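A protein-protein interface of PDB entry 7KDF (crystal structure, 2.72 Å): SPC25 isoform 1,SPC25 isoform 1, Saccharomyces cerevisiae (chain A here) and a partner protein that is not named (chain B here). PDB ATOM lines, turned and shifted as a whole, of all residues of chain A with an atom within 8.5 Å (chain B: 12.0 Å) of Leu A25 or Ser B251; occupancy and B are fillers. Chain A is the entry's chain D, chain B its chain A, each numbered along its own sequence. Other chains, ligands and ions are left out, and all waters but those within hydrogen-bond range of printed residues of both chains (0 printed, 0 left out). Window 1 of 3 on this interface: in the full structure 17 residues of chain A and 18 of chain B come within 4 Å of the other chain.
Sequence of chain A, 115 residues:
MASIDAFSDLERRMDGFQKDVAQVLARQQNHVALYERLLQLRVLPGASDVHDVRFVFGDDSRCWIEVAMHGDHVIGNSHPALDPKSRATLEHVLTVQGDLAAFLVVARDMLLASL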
ATOM      1  N   PHE A  17      -2.041  11.066  23.263  1.00  0.00           N
ATOM      2  CA  PHE A  17      -2.232  11.090  21.814  1.00  0.00           C
ATOM      3  C   PHE A  17      -1.475  12.247  21.178  1.00  0.00           C
ATOM      4  O   PHE A  17      -0.911  12.107  20.086  1.00  0.00           O
ATOM      5  CB  PHE A  17      -3.724  11.171  21.499  1.00  0.00           C
ATOM      6  CG  PHE A  17      -4.040  11.509  20.067  1.00  0.00           C
ATOM      7  CD1 PHE A  17      -4.205  10.508  19.127  1.00  0.00           C
ATOM      8  CD2 PHE A  17      -4.207  12.825  19.669  1.00  0.00           C
ATOM      9  CE1 PHE A  17      -4.509  10.814  17.816  1.00  0.00           C
ATOM     10  CE2 PHE A  17      -4.507  13.130  18.359  1.00  0.00           C
ATOM     11  CZ  PHE A  17      -4.658  12.126  17.433  1.00  0.00           C
ATOM     12  N   GLN A  18      -1.464  13.402  21.845  1.00  0.00           N
ATOM     13  CA  GLN A  18      -0.714  14.554  21.361  1.00  0.00           C
ATOM     14  C   GLN A  18       0.751  14.220  21.120  1.00  0.00           C
ATOM     15  O   GLN A  18       1.370  14.763  20.199  1.00  0.00           O
ATOM     16  CB  GLN A  18      -0.835  15.688  22.371  1.00  0.00           C
ATOM     17  CG  GLN A  18      -0.052  16.923  22.037  1.00  0.00           C
ATOM     18  CD  GLN A  18      -0.686  18.154  22.626  1.00  0.00           C
ATOM     19  OE1 GLN A  18      -1.494  18.071  23.554  1.00  0.00           O
ATOM     20  NE2 GLN A  18      -0.312  19.307  22.105  1.00  0.00           N
ATOM     21  N   LYS A  19       1.321  13.333  21.934  1.00  0.00           N
ATOM     22  CA  LYS A  19       2.709  12.937  21.768  1.00  0.00           C
ATOM     23  C   LYS A  19       2.867  11.717  20.872  1.00  0.00           C
ATOM     24  O   LYS A  19       3.963  11.491  20.348  1.00  0.00           O
ATOM     25  CB  LYS A  19       3.346  12.676  23.136  1.00  0.00           C
ATOM     26  CG  LYS A  19       3.193  13.850  24.097  1.00  0.00           C
ATOM     27  CD  LYS A  19       3.820  15.116  23.525  1.00  0.00           C
ATOM     28  CE  LYS A  19       3.579  16.325  24.421  1.00  0.00           C
ATOM     29  NZ  LYS A  19       4.133  17.569  23.818  1.00  0.00           N
ATOM     30  N   ASP A  20       1.804  10.933  20.682  1.00  0.00           N
ATOM     31  CA  ASP A  20       1.832   9.897  19.655  1.00  0.00           C
ATOM     32  C   ASP A  20       1.974  10.515  18.268  1.00  0.00           C
ATOM     33  O   ASP A  20       2.669   9.967  17.406  1.00  0.00           O
ATOM     34  CB  ASP A  20       0.575   9.034  19.738  1.00  0.00           C
ATOM     35  CG  ASP A  20       0.666   7.973  20.818  1.00  0.00           C
ATOM     36  OD1 ASP A  20       1.576   7.121  20.739  1.00  0.00           O
ATOM     37  OD2 ASP A  20      -0.173   7.994  21.743  1.00  0.00           O
ATOM     38  N   VAL A  21       1.311  11.652  18.036  1.00  0.00           N
ATOM     39  CA  VAL A  21       1.495  12.394  16.789  1.00  0.00           C
ATOM     40  C   VAL A  21       2.961  12.752  16.583  1.00  0.00           C
ATOM     41  O   VAL A  21       3.513  12.559  15.492  1.00  0.00           O
ATOM     42  CB  VAL A  21       0.603  13.647  16.774  1.00  0.00           C
ATOM     43  CG1 VAL A  21       0.994  14.548  15.628  1.00  0.00           C
ATOM     44  CG2 VAL A  21      -0.855  13.243  16.611  1.00  0.00           C
ATOM     45  N   ALA A  22       3.616  13.272  17.624  1.00  0.00           N
ATOM     46  CA  ALA A  22       5.015  13.664  17.485  1.00  0.00           C
ATOM     47  C   ALA A  22       5.884  12.479  17.075  1.00  0.00           C
ATOM     48  O   ALA A  22       6.817  12.631  16.277  1.00  0.00           O
ATOM     49  CB  ALA A  22       5.520  14.281  18.788  1.00  0.00           C
ATOM     50  N   GLN A  23       5.584  11.289  17.602  1.00  0.00           N
ATOM     51  CA  GLN A  23       6.339  10.097  17.231  1.00  0.00           C
ATOM     52  C   GLN A  23       6.141   9.752  15.762  1.00  0.00           C
ATOM     53  O   GLN A  23       7.108   9.491  15.036  1.00  0.00           O
ATOM     54  CB  GLN A  23       5.924   8.917  18.112  1.00  0.00           C
ATOM     55  CG  GLN A  23       6.432   8.991  19.537  1.00  0.00           C
ATOM     56  CD  GLN A  23       7.936   9.157  19.608  1.00  0.00           C
ATOM     57  OE1 GLN A  23       8.683   8.474  18.906  1.00  0.00           O
ATOM     58  NE2 GLN A  23       8.389  10.069  20.461  1.00  0.00           N
ATOM     59  N   VAL A  24       4.889   9.748  15.304  1.00  0.00           N
ATOM     60  CA  VAL A  24       4.600   9.356  13.928  1.00  0.00           C
ATOM     61  C   VAL A  24       5.203  10.355  12.949  1.00  0.00           C
ATOM     62  O   VAL A  24       5.641   9.985  11.853  1.00  0.00           O
ATOM     63  CB  VAL A  24       3.082   9.204  13.727  1.00  0.00           C
ATOM     64  CG1 VAL A  24       2.764   8.837  12.287  1.00  0.00           C
ATOM     65  CG2 VAL A  24       2.533   8.154  14.676  1.00  0.00           C
ATOM     66  N   LEU A  25       5.240  11.633  13.321  1.00  0.00           N
ATOM     67  CA  LEU A  25       5.706  12.666  12.412  1.00  0.00           C
ATOM     68  C   LEU A  25       7.189  12.976  12.608  1.00  0.00           C
ATOM     69  O   LEU A  25       7.649  14.043  12.183  1.00  0.00           O
ATOM     70  CB  LEU A  25       4.871  13.934  12.586  1.00  0.00           C
ATOM     71  CG  LEU A  25       3.350  13.770  12.427  1.00  0.00           C
ATOM     72  CD1 LEU A  25       2.628  15.111  12.584  1.00  0.00           C
ATOM     73  CD2 LEU A  25       2.910  13.009  11.181  1.00  0.00           C
ATOM     74  N   ALA A  26       7.936  12.069  13.246  1.00  0.00           N
ATOM     75  CA  ALA A  26       9.371  12.256  13.438  1.00  0.00           C
ATOM     76  C   ALA A  26      10.048  12.441  12.091  1.00  0.00           C
ATOM     77  O   ALA A  26       9.748  11.729  11.129  1.00  0.00           O
ATOM     78  CB  ALA A  26       9.975  11.059  14.171  1.00  0.00           C
ATOM     79  N   ARG A  27      10.967  13.403  12.021  1.00  0.00           N
ATOM     80  CA  ARG A  27      11.283  13.997  10.728  1.00  0.00           C
ATOM     81  C   ARG A  27      12.048  12.946   9.938  1.00  0.00           C
ATOM     82  O   ARG A  27      13.238  12.722  10.174  1.00  0.00           O
ATOM     83  CB  ARG A  27      12.131  15.257  10.855  1.00  0.00           C
ATOM     84  CG  ARG A  27      11.992  16.111   9.596  1.00  0.00           C
ATOM     85  CD  ARG A  27      12.947  17.298   9.461  1.00  0.00           C
ATOM     86  NE  ARG A  27      12.994  18.215  10.589  1.00  0.00           N
ATOM     87  CZ  ARG A  27      13.784  19.285  10.617  1.00  0.00           C
ATOM     88  NH1 ARG A  27      14.464  19.638   9.521  1.00  0.00           N
ATOM     89  NH2 ARG A  27      13.831  20.055  11.702  1.00  0.00           N
ATOM     90  N   GLN A  28      11.365  12.269   9.020  1.00  0.00           N
ATOM     91  CA  GLN A  28      12.028  11.244   8.226  1.00  0.00           C
ATOM     92  C   GLN A  28      13.148  11.870   7.406  1.00  0.00           C
ATOM     93  O   GLN A  28      12.940  12.862   6.701  1.00  0.00           O
ATOM     94  CB  GLN A  28      11.021  10.544   7.314  1.00  0.00           C
ATOM     95  CG  GLN A  28      11.578   9.317   6.608  1.00  0.00           C
ATOM     96  CD  GLN A  28      11.007   9.137   5.213  1.00  0.00           C
ATOM     97  OE1 GLN A  28      10.578  10.099   4.576  1.00  0.00           O
ATOM     98  NE2 GLN A  28      10.998   7.899   4.732  1.00  0.00           N
ATOM     99  N   SER B 242      -8.811  23.549  23.165  1.00  0.00           N
ATOM    100  CA  SER B 242      -8.337  24.418  22.095  1.00  0.00           C
ATOM    101  C   SER B 242      -6.825  24.323  21.937  1.00  0.00           C
ATOM    102  O   SER B 242      -6.316  24.255  20.812  1.00  0.00           O
ATOM    103  CB  SER B 242      -8.763  25.859  22.365  1.00  0.00           C
ATOM    104  OG  SER B 242      -8.167  26.343  23.553  1.00  0.00           O
ATOM    105  N   LYS B 243      -6.090  24.317  23.052  1.00  0.00           N
ATOM    106  CA  LYS B 243      -4.637  24.190  22.967  1.00  0.00           C
ATOM    107  C   LYS B 243      -4.246  22.853  22.350  1.00  0.00           C
ATOM    108  O   LYS B 243      -3.296  22.776  21.564  1.00  0.00           O
ATOM    109  CB  LYS B 243      -4.000  24.356  24.351  1.00  0.00           C
ATOM    110  CG  LYS B 243      -2.482  24.235  24.323  1.00  0.00           C
ATOM    111  CD  LYS B 243      -1.814  24.648  25.625  1.00  0.00           C
ATOM    112  CE  LYS B 243      -0.291  24.582  25.480  1.00  0.00           C
ATOM    113  NZ  LYS B 243       0.441  25.073  26.685  1.00  0.00           N
ATOM    114  N   PHE B 244      -4.976  21.792  22.697  1.00  0.00           N
ATOM    115  CA  PHE B 244      -4.760  20.485  22.089  1.00  0.00           C
ATOM    116  C   PHE B 244      -4.903  20.549  20.571  1.00  0.00           C
ATOM    117  O   PHE B 244      -3.998  20.141  19.832  1.00  0.00           O
ATOM    118  CB  PHE B 244      -5.751  19.498  22.708  1.00  0.00           C
ATOM    119  CG  PHE B 244      -5.821  18.160  22.038  1.00  0.00           C
ATOM    120  CD1 PHE B 244      -4.844  17.202  22.255  1.00  0.00           C
ATOM    121  CD2 PHE B 244      -6.905  17.836  21.239  1.00  0.00           C
ATOM    122  CE1 PHE B 244      -4.933  15.959  21.659  1.00  0.00           C
ATOM    123  CE2 PHE B 244      -7.001  16.598  20.638  1.00  0.00           C
ATOM    124  CZ  PHE B 244      -6.013  15.657  20.847  1.00  0.00           C
ATOM    125  N   LYS B 245      -6.023  21.096  20.086  1.00  0.00           N
ATOM    126  CA  LYS B 245      -6.305  21.068  18.655  1.00  0.00           C
ATOM    127  C   LYS B 245      -5.313  21.913  17.873  1.00  0.00           C
ATOM    128  O   LYS B 245      -4.813  21.485  16.822  1.00  0.00           O
ATOM    129  CB  LYS B 245      -7.736  21.538  18.394  1.00  0.00           C
ATOM    130  CG  LYS B 245      -8.205  21.274  16.974  1.00  0.00           C
ATOM    131  CD  LYS B 245      -7.909  19.841  16.561  1.00  0.00           C
ATOM    132  CE  LYS B 245      -8.885  19.353  15.505  1.00  0.00           C
ATOM    133  NZ  LYS B 245      -8.910  20.237  14.309  1.00  0.00           N
ATOM    134  N   ILE B 246      -5.004  23.109  18.379  1.00  0.00           N
ATOM    135  CA  ILE B 246      -4.070  23.987  17.684  1.00  0.00           C
ATOM    136  C   ILE B 246      -2.672  23.381  17.660  1.00  0.00           C
ATOM    137  O   ILE B 246      -1.934  23.527  16.678  1.00  0.00           O
ATOM    138  CB  ILE B 246      -4.084  25.398  18.307  1.00  0.00           C
ATOM    139  CG1 ILE B 246      -5.467  26.021  18.095  1.00  0.00           C
ATOM    140  CG2 ILE B 246      -2.941  26.269  17.788  1.00  0.00           C
ATOM    141  CD1 ILE B 246      -5.702  27.339  18.803  1.00  0.00           C
ATOM    142  N   ASN B 247      -2.279  22.700  18.739  1.00  0.00           N
ATOM    143  CA  ASN B 247      -0.931  22.141  18.796  1.00  0.00           C
ATOM    144  C   ASN B 247      -0.746  21.027  17.774  1.00  0.00           C
ATOM    145  O   ASN B 247       0.287  20.970  17.092  1.00  0.00           O
ATOM    146  CB  ASN B 247      -0.628  21.643  20.207  1.00  0.00           C
ATOM    147  CG  ASN B 247      -0.085  22.744  21.116  1.00  0.00           C
ATOM    148  OD1 ASN B 247       0.170  23.863  20.667  1.00  0.00           O
ATOM    149  ND2 ASN B 247       0.099  22.427  22.396  1.00  0.00           N
ATOM    150  N   ILE B 248      -1.735  20.137  17.649  1.00  0.00           N
ATOM    151  CA  ILE B 248      -1.650  19.080  16.644  1.00  0.00           C
ATOM    152  C   ILE B 248      -1.776  19.654  15.244  1.00  0.00           C
ATOM    153  O   ILE B 248      -1.155  19.155  14.298  1.00  0.00           O
ATOM    154  CB  ILE B 248      -2.689  17.975  16.912  1.00  0.00           C
ATOM    155  CG1 ILE B 248      -2.343  17.295  18.234  1.00  0.00           C
ATOM    156  CG2 ILE B 248      -2.804  17.003  15.729  1.00  0.00           C
ATOM    157  CD1 ILE B 248      -3.358  16.318  18.715  1.00  0.00           C
ATOM    158  N   GLN B 249      -2.597  20.694  15.077  1.00  0.00           N
ATOM    159  CA  GLN B 249      -2.643  21.369  13.787  1.00  0.00           C
ATOM    160  C   GLN B 249      -1.262  21.870  13.392  1.00  0.00           C
ATOM    161  O   GLN B 249      -0.872  21.782  12.221  1.00  0.00           O
ATOM    162  CB  GLN B 249      -3.647  22.517  13.820  1.00  0.00           C
ATOM    163  CG  GLN B 249      -5.049  22.090  13.440  1.00  0.00           C
ATOM    164  CD  GLN B 249      -6.039  23.233  13.485  1.00  0.00           C
ATOM    165  OE1 GLN B 249      -5.922  24.135  14.315  1.00  0.00           O
ATOM    166  NE2 GLN B 249      -7.035  23.191  12.602  1.00  0.00           N
ATOM    167  N   SER B 250      -0.501  22.381  14.362  1.00  0.00           N
ATOM    168  CA  SER B 250       0.875  22.786  14.097  1.00  0.00           C
ATOM    169  C   SER B 250       1.738  21.593  13.698  1.00  0.00           C
ATOM    170  O   SER B 250       2.542  21.684  12.761  1.00  0.00           O
ATOM    171  CB  SER B 250       1.452  23.484  15.329  1.00  0.00           C
ATOM    172  OG  SER B 250       2.840  23.728  15.181  1.00  0.00           O
ATOM    173  N   SER B 251       1.590  20.465  14.396  1.00  0.00           N
ATOM    174  CA  SER B 251       2.393  19.292  14.064  1.00  0.00           C
ATOM    175  C   SER B 251       2.092  18.803  12.654  1.00  0.00           C
ATOM    176  O   SER B 251       3.010  18.474  11.893  1.00  0.00           O
ATOM    177  CB  SER B 251       2.145  18.176  15.079  1.00  0.00           C
ATOM    178  OG  SER B 251       2.837  18.427  16.290  1.00  0.00           O
ATOM    179  N   LEU B 252       0.808  18.760  12.290  1.00  0.00           N
ATOM    180  CA  LEU B 252       0.420  18.329  10.953  1.00  0.00           C
ATOM    181  C   LEU B 252       0.973  19.271   9.892  1.00  0.00           C
ATOM    182  O   LEU B 252       1.462  18.827   8.846  1.00  0.00           O
ATOM    183  CB  LEU B 252      -1.103  18.249  10.862  1.00  0.00           C
ATOM    184  CG  LEU B 252      -1.796  17.134  11.647  1.00  0.00           C
ATOM    185  CD1 LEU B 252      -3.296  17.355  11.648  1.00  0.00           C
ATOM    186  CD2 LEU B 252      -1.458  15.759  11.080  1.00  0.00           C
ATOM    187  N   GLU B 253       0.902  20.580  10.146  1.00  0.00           N
ATOM    188  CA  GLU B 253       1.384  21.567   9.186  1.00  0.00           C
ATOM    189  C   GLU B 253       2.892  21.468   8.988  1.00  0.00           C
ATOM    190  O   GLU B 253       3.381  21.544   7.855  1.00  0.00           O
ATOM    191  CB  GLU B 253       0.986  22.965   9.656  1.00  0.00           C
ATOM    192  CG  GLU B 253       1.106  24.063   8.617  1.00  0.00           C
ATOM    193  CD  GLU B 253       0.959  25.447   9.236  1.00  0.00           C
ATOM    194  OE1 GLU B 253       0.939  25.542  10.484  1.00  0.00           O
ATOM    195  OE2 GLU B 253       0.860  26.436   8.479  1.00  0.00           O
ATOM    196  N   ASN B 254       3.647  21.303  10.076  1.00  0.00           N
ATOM    197  CA  ASN B 254       5.099  21.223   9.959  1.00  0.00           C
ATOM    198  C   ASN B 254       5.527  19.980   9.190  1.00  0.00           C
ATOM    199  O   ASN B 254       6.435  20.043   8.354  1.00  0.00           O
ATOM    200  CB  ASN B 254       5.738  21.247  11.347  1.00  0.00           C
ATOM    201  CG  ASN B 254       5.766  22.638  11.946  1.00  0.00           C
ATOM    202  OD1 ASN B 254       5.670  23.635  11.230  1.00  0.00           O
ATOM    203  ND2 ASN B 254       5.889  22.714  13.267  1.00  0.00           N
ATOM    204  N   SER B 255       4.882  18.842   9.456  1.00  0.00           N
ATOM    205  CA  SER B 255       5.265  17.605   8.783  1.00  0.00           C
ATOM    206  C   SER B 255       5.043  17.701   7.279  1.00  0.00           C
ATOM    207  O   SER B 255       5.876  17.241   6.488  1.00  0.00           O
ATOM    208  CB  SER B 255       4.481  16.431   9.370  1.00  0.00           C
ATOM    209  OG  SER B 255       4.725  15.241   8.640  1.00  0.00           O
ATOM    210  N   GLU B 256       3.920  18.297   6.867  1.00  0.00           N
ATOM    211  CA  GLU B 256       3.575  18.351   5.450  1.00  0.00           C
ATOM    212  C   GLU B 256       4.550  19.220   4.659  1.00  0.00           C
ATOM    213  O   GLU B 256       4.998  18.812   3.575  1.00  0.00           O
ATOM    214  CB  GLU B 256       2.132  18.834   5.299  1.00  0.00           C
ATOM    215  CG  GLU B 256       1.449  18.354   4.038  1.00  0.00           C
ATOM    216  CD  GLU B 256      -0.034  18.660   4.010  1.00  0.00           C
ATOM    217  OE1 GLU B 256      -0.518  19.385   4.905  1.00  0.00           O
ATOM    218  OE2 GLU B 256      -0.711  18.195   3.069  1.00  0.00           O
ATOM    219  N   ASN B 257       4.893  20.412   5.184  1.00  0.00           N
ATOM    220  CA  ASN B 257       5.973  21.196   4.589  1.00  0.00           C
ATOM    221  C   ASN B 257       7.312  20.470   4.637  1.00  0.00           C
ATOM    222  O   ASN B 257       8.099  20.586   3.690  1.00  0.00           O
ATOM    223  CB  ASN B 257       6.084  22.576   5.234  1.00  0.00           C
ATOM    224  CG  ASN B 257       4.937  23.497   4.865  1.00  0.00           C
ATOM    225  OD1 ASN B 257       4.110  23.875   5.697  1.00  0.00           O
ATOM    226  ND2 ASN B 257       4.966  23.966   3.611  1.00  0.00           N
ATOM    227  N   GLU B 258       7.608  19.737   5.716  1.00  0.00           N
ATOM    228  CA  GLU B 258       8.849  18.978   5.738  1.00  0.00           C
ATOM    229  C   GLU B 258       8.904  18.021   4.559  1.00  0.00           C
ATOM    230  O   GLU B 258       9.871  18.020   3.791  1.00  0.00           O
ATOM    231  CB  GLU B 258       8.983  18.222   7.058  1.00  0.00           C
ATOM    232  CG  GLU B 258       9.571  19.032   8.190  1.00  0.00           C
ATOM    233  CD  GLU B 258       9.204  18.470   9.546  1.00  0.00           C
ATOM    234  OE1 GLU B 258       9.042  19.271  10.490  1.00  0.00           O
ATOM    235  OE2 GLU B 258       9.048  17.236   9.661  1.00  0.00           O
ATOM    236  N   LEU B 259       7.858  17.213   4.390  1.00  0.00           N
ATOM    237  CA  LEU B 259       7.896  16.166   3.379  1.00  0.00           C
ATOM    238  C   LEU B 259       7.771  16.735   1.974  1.00  0.00           C
ATOM    239  O   LEU B 259       8.304  16.153   1.024  1.00  0.00           O
ATOM    240  CB  LEU B 259       6.795  15.149   3.657  1.00  0.00           C
ATOM    241  CG  LEU B 259       6.975  14.463   5.015  1.00  0.00           C
ATOM    242  CD1 LEU B 259       5.857  13.471   5.296  1.00  0.00           C
ATOM    243  CD2 LEU B 259       8.341  13.802   5.132  1.00  0.00           C
ATOM    244  N   GLY B 260       7.086  17.870   1.822  1.00  0.00           N
ATOM    245  CA  GLY B 260       7.058  18.532   0.529  1.00  0.00           C
ATOM    246  C   GLY B 260       8.440  18.936   0.057  1.00  0.00           C
ATOM    247  O   GLY B 260       8.774  18.788  -1.121  1.00  0.00           O
ATOM    248  N   VAL B 262      11.230  17.485   0.911  1.00  0.00           N
ATOM    249  CA  VAL B 262      11.927  16.258   0.540  1.00  0.00           C
ATOM    250  C   VAL B 262      11.558  15.855  -0.881  1.00  0.00           C
ATOM    251  O   VAL B 262      12.422  15.487  -1.685  1.00  0.00           O
ATOM    252  CB  VAL B 262      11.611  15.138   1.548  1.00  0.00           C
ATOM    253  CG1 VAL B 262      12.218  13.814   1.092  1.00  0.00           C
ATOM    254  CG2 VAL B 262      12.109  15.518   2.931  1.00  0.00           C
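Hydrophobic or aromatic side chains of chain A within 4 Å of the printed part of chain B: Phe A17, Val A21 and Leu A25.
Along chain A the printed residues that touch a printed residue of chain B span positions 17 to 27.
Printed residues of chain B that touch a printed residue of chain A: Phe B244, Asn B247, Ile B248, Ser B251, Ser B255 and Glu B258.
Hydrophobic or aromatic side chains of chain B that line the printed part of chain A: Phe B244 and Ile B248.
The side-chain amide nitrogen (ND2) of Asn B247 lies close to the side-chain amide nitrogen (NE2) of Gln A18, at 3.2 Å.
Phe A17 touches Phe B244.
CD1 of Ile B248 touches CE2 of Phe A17, at 3.4 Å.
OE1 of Gln A18 touches CD1 of Phe B244, at 3.7 Å.
Val A21 touches Ser B251 (CG1 to CB, 3.8 Å).
Ser B251 touches Leu A25.
CD2 of Leu A25 touches OG of Ser B255 (3.8 Å).
OE2 of Glu B258 touches CG of Arg A27, at 3.2 Å.
Of chain B, only Ser B251 comes within 4 Å of Val A21.
Leu A25 touches two residues of chain B.
No residue of chain B comes within 4 Å of Ala A26.
Ser B242 touches none of the printed residues of chain A.
Of the printed residues of chain A, Asn B247 touches Gln A18 (3.0 Å).
No residue of chain A comes within 4 Å of Ser B250.
Of the printed residues of chain A, Ser B255 touches Leu A25 (3.8 Å).
Printed residues of chain A within 4 Å of Glu B258: Arg A27 (3.2 Å).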
